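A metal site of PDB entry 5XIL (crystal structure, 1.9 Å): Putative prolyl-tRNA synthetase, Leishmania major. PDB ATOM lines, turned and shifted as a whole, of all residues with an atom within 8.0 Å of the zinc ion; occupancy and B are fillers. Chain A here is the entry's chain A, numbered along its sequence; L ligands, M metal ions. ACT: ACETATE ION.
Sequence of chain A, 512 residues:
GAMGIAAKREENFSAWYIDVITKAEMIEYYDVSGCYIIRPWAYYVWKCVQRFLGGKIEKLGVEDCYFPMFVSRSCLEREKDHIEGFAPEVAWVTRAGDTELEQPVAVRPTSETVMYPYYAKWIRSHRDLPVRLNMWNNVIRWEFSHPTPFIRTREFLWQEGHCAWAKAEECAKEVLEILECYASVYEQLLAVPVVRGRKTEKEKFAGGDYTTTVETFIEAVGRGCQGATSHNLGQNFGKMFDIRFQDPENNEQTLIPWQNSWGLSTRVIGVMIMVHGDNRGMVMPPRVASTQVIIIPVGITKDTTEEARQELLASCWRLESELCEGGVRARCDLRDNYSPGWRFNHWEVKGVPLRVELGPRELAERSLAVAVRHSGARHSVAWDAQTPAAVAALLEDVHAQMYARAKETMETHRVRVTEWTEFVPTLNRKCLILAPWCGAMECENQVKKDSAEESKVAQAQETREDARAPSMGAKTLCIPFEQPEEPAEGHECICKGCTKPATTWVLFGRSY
Within 4 Å of the zinc ion: Cys 438, Cys 443 and Cys 493.
The zinc ion is bound by O of the ligand (2.1 Å), SG of Cys 443 (2.2 Å), SG of Cys 438 (2.3 Å) and SG of Cys 493 (2.4 Å).
SG of Cys 438 sits close to N of Ala 440, at 3.5 Å. N of Cys 493 lies within hydrogen-bond range of O of Lys 500, 2.8 Å away. SG of Cys 495 forms a disulfide with SG of Cys 498. The side-chain sulfur (SG) of Cys 443 sits close to the side-chain sulfur (SG) of Cys 495 (3.5 Å). OG1 of Thr 503 is in hydrogen-bond range of O of Cys 438 (3.0 Å).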
ATOM      1  N   PRO A 436     -11.878  29.163 -14.446  1.00  0.00           N
ATOM      2  CA  PRO A 436     -10.769  28.334 -14.932  1.00  0.00           C
ATOM      3  C   PRO A 436     -11.068  26.919 -14.587  1.00  0.00           C
ATOM      4  O   PRO A 436     -11.572  26.642 -13.488  1.00  0.00           O
ATOM      5  CB  PRO A 436      -9.561  28.783 -14.113  1.00  0.00           C
ATOM      6  CG  PRO A 436      -9.950  30.118 -13.544  1.00  0.00           C
ATOM      7  CD  PRO A 436     -11.441  30.107 -13.383  1.00  0.00           C
ATOM      8  N   TRP A 437     -10.777  25.995 -15.501  1.00  0.00           N
ATOM      9  CA  TRP A 437     -11.087  24.558 -15.299  1.00  0.00           C
ATOM     10  C   TRP A 437      -9.920  23.722 -15.848  1.00  0.00           C
ATOM     11  O   TRP A 437      -9.324  24.108 -16.851  1.00  0.00           O
ATOM     12  CB  TRP A 437     -12.354  24.232 -16.061  1.00  0.00           C
ATOM     13  CG  TRP A 437     -12.845  22.824 -15.966  1.00  0.00           C
ATOM     14  CD1 TRP A 437     -12.868  22.017 -14.855  1.00  0.00           C
ATOM     15  CD2 TRP A 437     -13.363  22.036 -17.030  1.00  0.00           C
ATOM     16  NE1 TRP A 437     -13.416  20.783 -15.167  1.00  0.00           N
ATOM     17  CE2 TRP A 437     -13.719  20.769 -16.487  1.00  0.00           C
ATOM     18  CE3 TRP A 437     -13.524  22.259 -18.374  1.00  0.00           C
ATOM     19  CZ2 TRP A 437     -14.285  19.773 -17.255  1.00  0.00           C
ATOM     20  CZ3 TRP A 437     -14.099  21.281 -19.104  1.00  0.00           C
ATOM     21  CH2 TRP A 437     -14.465  20.042 -18.567  1.00  0.00           C
ATOM     22  N   CYS A 438      -9.518  22.647 -15.156  1.00  0.00           N
ATOM     23  CA  CYS A 438      -8.388  21.834 -15.679  1.00  0.00           C
ATOM     24  C   CYS A 438      -8.843  20.886 -16.775  1.00  0.00           C
ATOM     25  O   CYS A 438      -8.022  20.347 -17.546  1.00  0.00           O
ATOM     26  CB  CYS A 438      -7.714  21.007 -14.545  1.00  0.00           C
ATOM     27  SG  CYS A 438      -8.810  19.807 -13.795  1.00  0.00           S
ATOM     28  N   GLY A 439     -10.143  20.668 -16.862  1.00  0.00           N
ATOM     29  CA  GLY A 439     -10.716  19.816 -17.850  1.00  0.00           C
ATOM     30  C   GLY A 439     -11.149  18.474 -17.331  1.00  0.00           C
ATOM     31  O   GLY A 439     -11.703  17.663 -18.093  1.00  0.00           O
ATOM     32  N   ALA A 440     -10.910  18.183 -16.047  1.00  0.00           N
ATOM     33  CA  ALA A 440     -11.321  16.886 -15.489  1.00  0.00           C
ATOM     34  C   ALA A 440     -12.788  16.815 -15.180  1.00  0.00           C
ATOM     35  O   ALA A 440     -13.325  17.733 -14.548  1.00  0.00           O
ATOM     36  CB  ALA A 440     -10.522  16.598 -14.218  1.00  0.00           C
ATOM     37  N   MET A 441     -13.460  15.740 -15.585  1.00  0.00           N
ATOM     38  CA  MET A 441     -14.877  15.554 -15.239  1.00  0.00           C
ATOM     39  C   MET A 441     -15.177  15.578 -13.775  1.00  0.00           C
ATOM     40  O   MET A 441     -16.234  16.069 -13.319  1.00  0.00           O
ATOM     41  CB  MET A 441     -15.413  14.232 -15.821  1.00  0.00           C
ATOM     42  CG  MET A 441     -16.909  14.185 -15.904  1.00  0.00           C
ATOM     43  SD  MET A 441     -17.452  12.645 -16.639  1.00  0.00           S
ATOM     44  CE  MET A 441     -17.093  12.961 -18.359  1.00  0.00           C
ATOM     45  N   GLU A 442     -14.273  15.005 -12.980  1.00  0.00           N
ATOM     46  CA  GLU A 442     -14.427  14.983 -11.540  1.00  0.00           C
ATOM     47  C   GLU A 442     -14.638  16.405 -10.943  1.00  0.00           C
ATOM     48  O   GLU A 442     -15.420  16.629 -10.020  1.00  0.00           O
ATOM     49  CB  GLU A 442     -13.155  14.358 -10.927  1.00  0.00           C
ATOM     50  CG  GLU A 442     -12.825  12.996 -11.531  1.00  0.00           C
ATOM     51  CD  GLU A 442     -11.736  13.063 -12.608  1.00  0.00           C
ATOM     52  OE1 GLU A 442     -10.562  12.788 -12.262  1.00  0.00           O
ATOM     53  OE2 GLU A 442     -12.049  13.335 -13.784  1.00  0.00           O
ATOM     54  N   CYS A 443     -13.892  17.358 -11.490  1.00  0.00           N
ATOM     55  CA  CYS A 443     -13.919  18.742 -11.026  1.00  0.00           C
ATOM     56  C   CYS A 443     -15.239  19.410 -11.380  1.00  0.00           C
ATOM     57  O   CYS A 443     -15.836  20.088 -10.538  1.00  0.00           O
ATOM     58  CB  CYS A 443     -12.762  19.528 -11.582  1.00  0.00           C
ATOM     59  SG  CYS A 443     -11.084  18.936 -11.032  1.00  0.00           S
ATOM     60  N   GLU A 444     -15.700  19.172 -12.599  1.00  0.00           N
ATOM     61  CA  GLU A 444     -17.065  19.608 -13.008  1.00  0.00           C
ATOM     62  C   GLU A 444     -18.137  19.059 -12.101  1.00  0.00           C
ATOM     63  O   GLU A 444     -19.083  19.774 -11.704  1.00  0.00           O
ATOM     64  CB  GLU A 444     -17.301  19.171 -14.461  1.00  0.00           C
ATOM     65  CG  GLU A 444     -18.638  19.455 -15.036  1.00  0.00           C
ATOM     66  CD  GLU A 444     -18.660  19.146 -16.544  1.00  0.00           C
ATOM     67  OE1 GLU A 444     -17.635  18.594 -17.100  1.00  0.00           O
ATOM     68  OE2 GLU A 444     -19.694  19.475 -17.177  1.00  0.00           O
ATOM     69  N   GLN A 446     -17.744  18.058  -8.940  1.00  0.00           N
ATOM     70  CA  GLN A 446     -17.569  18.659  -7.642  1.00  0.00           C
ATOM     71  C   GLN A 446     -18.177  20.095  -7.604  1.00  0.00           C
ATOM     72  O   GLN A 446     -18.883  20.468  -6.684  1.00  0.00           O
ATOM     73  CB  GLN A 446     -16.103  18.746  -7.290  1.00  0.00           C
ATOM     74  CG  GLN A 446     -15.915  18.977  -5.787  1.00  0.00           C
ATOM     75  CD  GLN A 446     -14.538  19.387  -5.414  1.00  0.00           C
ATOM     76  OE1 GLN A 446     -13.541  18.794  -5.865  1.00  0.00           O
ATOM     77  NE2 GLN A 446     -14.438  20.421  -4.577  1.00  0.00           N
ATOM     78  N   VAL A 447     -17.928  20.861  -8.667  1.00  0.00           N
ATOM     79  CA  VAL A 447     -18.556  22.199  -8.754  1.00  0.00           C
ATOM     80  C   VAL A 447     -20.077  22.107  -8.594  1.00  0.00           C
ATOM     81  O   VAL A 447     -20.675  22.875  -7.826  1.00  0.00           O
ATOM     82  CB  VAL A 447     -18.143  22.904 -10.028  1.00  0.00           C
ATOM     83  CG1 VAL A 447     -19.010  24.159 -10.247  1.00  0.00           C
ATOM     84  CG2 VAL A 447     -16.658  23.234  -9.981  1.00  0.00           C
ATOM     85  N   GLU A 492      -5.519  28.324 -10.814  1.00  0.00           N
ATOM     86  CA  GLU A 492      -5.905  26.997 -10.459  1.00  0.00           C
ATOM     87  C   GLU A 492      -7.287  26.661 -10.930  1.00  0.00           C
ATOM     88  O   GLU A 492      -8.142  27.532 -11.069  1.00  0.00           O
ATOM     89  CB  GLU A 492      -5.898  26.824  -8.946  1.00  0.00           C
ATOM     90  CG  GLU A 492      -4.520  27.072  -8.364  1.00  0.00           C
ATOM     91  CD  GLU A 492      -4.140  28.581  -8.392  1.00  0.00           C
ATOM     92  OE1 GLU A 492      -5.027  29.480  -8.192  1.00  0.00           O
ATOM     93  OE2 GLU A 492      -2.968  28.877  -8.686  1.00  0.00           O
ATOM     94  N   CYS A 493      -7.527  25.381 -11.187  1.00  0.00           N
ATOM     95  CA  CYS A 493      -8.910  24.940 -11.427  1.00  0.00           C
ATOM     96  C   CYS A 493      -9.874  25.433 -10.325  1.00  0.00           C
ATOM     97  O   CYS A 493      -9.524  25.493  -9.164  1.00  0.00           O
ATOM     98  CB  CYS A 493      -8.890  23.432 -11.598  1.00  0.00           C
ATOM     99  SG  CYS A 493     -10.461  22.662 -11.806  1.00  0.00           S
ATOM    100  N   ILE A 494     -11.115  25.812 -10.698  1.00  0.00           N
ATOM    101  CA  ILE A 494     -12.019  26.526  -9.781  1.00  0.00           C
ATOM    102  C   ILE A 494     -12.528  25.763  -8.589  1.00  0.00           C
ATOM    103  O   ILE A 494     -12.907  26.393  -7.570  1.00  0.00           O
ATOM    104  CB  ILE A 494     -13.243  27.137 -10.561  1.00  0.00           C
ATOM    105  CG1 ILE A 494     -14.058  28.160  -9.709  1.00  0.00           C
ATOM    106  CG2 ILE A 494     -14.117  25.974 -11.063  1.00  0.00           C
ATOM    107  CD1 ILE A 494     -13.213  29.276  -9.110  1.00  0.00           C
ATOM    108  N   CYS A 495     -12.617  24.433  -8.660  1.00  0.00           N
ATOM    109  CA  CYS A 495     -13.284  23.680  -7.639  1.00  0.00           C
ATOM    110  C   CYS A 495     -12.582  23.832  -6.281  1.00  0.00           C
ATOM    111  O   CYS A 495     -11.392  24.102  -6.192  1.00  0.00           O
ATOM    112  CB  CYS A 495     -13.554  22.188  -7.929  1.00  0.00           C
ATOM    113  SG  CYS A 495     -12.198  21.303  -8.676  1.00  0.00           S
ATOM    114  N   CYS A 498      -9.223  22.577  -5.169  1.00  0.00           N
ATOM    115  CA  CYS A 498      -8.497  22.081  -6.349  1.00  0.00           C
ATOM    116  C   CYS A 498      -7.248  22.842  -6.509  1.00  0.00           C
ATOM    117  O   CYS A 498      -7.142  23.934  -5.981  1.00  0.00           O
ATOM    118  CB  CYS A 498      -9.364  22.090  -7.626  1.00  0.00           C
ATOM    119  SG  CYS A 498     -10.727  20.996  -7.270  1.00  0.00           S
ATOM    120  N   THR A 499      -6.285  22.222  -7.193  1.00  0.00           N
ATOM    121  CA  THR A 499      -4.909  22.661  -7.244  1.00  0.00           C
ATOM    122  C   THR A 499      -4.276  22.648  -8.599  1.00  0.00           C
ATOM    123  O   THR A 499      -3.285  23.331  -8.807  1.00  0.00           O
ATOM    124  CB  THR A 499      -4.040  21.736  -6.336  1.00  0.00           C
ATOM    125  OG1 THR A 499      -4.400  22.005  -4.972  1.00  0.00           O
ATOM    126  CG2 THR A 499      -2.574  22.005  -6.489  1.00  0.00           C
ATOM    127  N   LYS A 500      -4.756  21.810  -9.511  1.00  0.00           N
ATOM    128  CA  LYS A 500      -4.162  21.758 -10.835  1.00  0.00           C
ATOM    129  C   LYS A 500      -4.313  23.038 -11.579  1.00  0.00           C
ATOM    130  O   LYS A 500      -5.361  23.703 -11.453  1.00  0.00           O
ATOM    131  CB  LYS A 500      -4.790  20.624 -11.682  1.00  0.00           C
ATOM    132  CG  LYS A 500      -4.425  19.283 -11.119  1.00  0.00           C
ATOM    133  CD  LYS A 500      -5.137  18.144 -11.829  1.00  0.00           C
ATOM    134  CE  LYS A 500      -4.502  16.826 -11.391  1.00  0.00           C
ATOM    135  NZ  LYS A 500      -5.365  15.711 -11.842  1.00  0.00           N
ATOM    136  N   PRO A 501      -3.288  23.401 -12.388  1.00  0.00           N
ATOM    137  CA  PRO A 501      -3.446  24.512 -13.308  1.00  0.00           C
ATOM    138  C   PRO A 501      -4.622  24.253 -14.262  1.00  0.00           C
ATOM    139  O   PRO A 501      -4.846  23.142 -14.762  1.00  0.00           O
ATOM    140  CB  PRO A 501      -2.109  24.567 -14.091  1.00  0.00           C
ATOM    141  CG  PRO A 501      -1.209  23.600 -13.378  1.00  0.00           C
ATOM    142  CD  PRO A 501      -2.045  22.645 -12.623  1.00  0.00           C
ATOM    143  N   ALA A 502      -5.444  25.288 -14.446  1.00  0.00           N
ATOM    144  CA  ALA A 502      -6.502  25.254 -15.436  1.00  0.00           C
ATOM    145  C   ALA A 502      -5.923  25.217 -16.854  1.00  0.00           C
ATOM    146  O   ALA A 502      -4.827  25.775 -17.147  1.00  0.00           O
ATOM    147  CB  ALA A 502      -7.373  26.481 -15.269  1.00  0.00           C
ATOM    148  N   THR A 503      -6.677  24.630 -17.758  1.00  0.00           N
ATOM    149  CA  THR A 503      -6.366  24.653 -19.170  1.00  0.00           C
ATOM    150  C   THR A 503      -7.314  25.437 -20.032  1.00  0.00           C
ATOM    151  O   THR A 503      -6.999  25.705 -21.186  1.00  0.00           O
ATOM    152  CB  THR A 503      -6.320  23.204 -19.727  1.00  0.00           C
ATOM    153  OG1 THR A 503      -7.591  22.573 -19.531  1.00  0.00           O
ATOM    154  CG2 THR A 503      -5.254  22.400 -18.927  1.00  0.00           C
HETATM  155  C   ACT L   1      -7.693  19.675  -9.530  1.00  0.00           C
HETATM  156  O   ACT L   1      -8.065  20.556 -10.337  1.00  0.00           O
HETATM  157  OXT ACT L   1      -6.908  19.966  -8.524  1.00  0.00           O
HETATM  158  CH3 ACT L   1      -8.200  18.279  -9.784  1.00  0.00           C
HETATM  159 ZN    ZN M   1      -9.639  20.435 -11.740  1.00  0.00          ZN
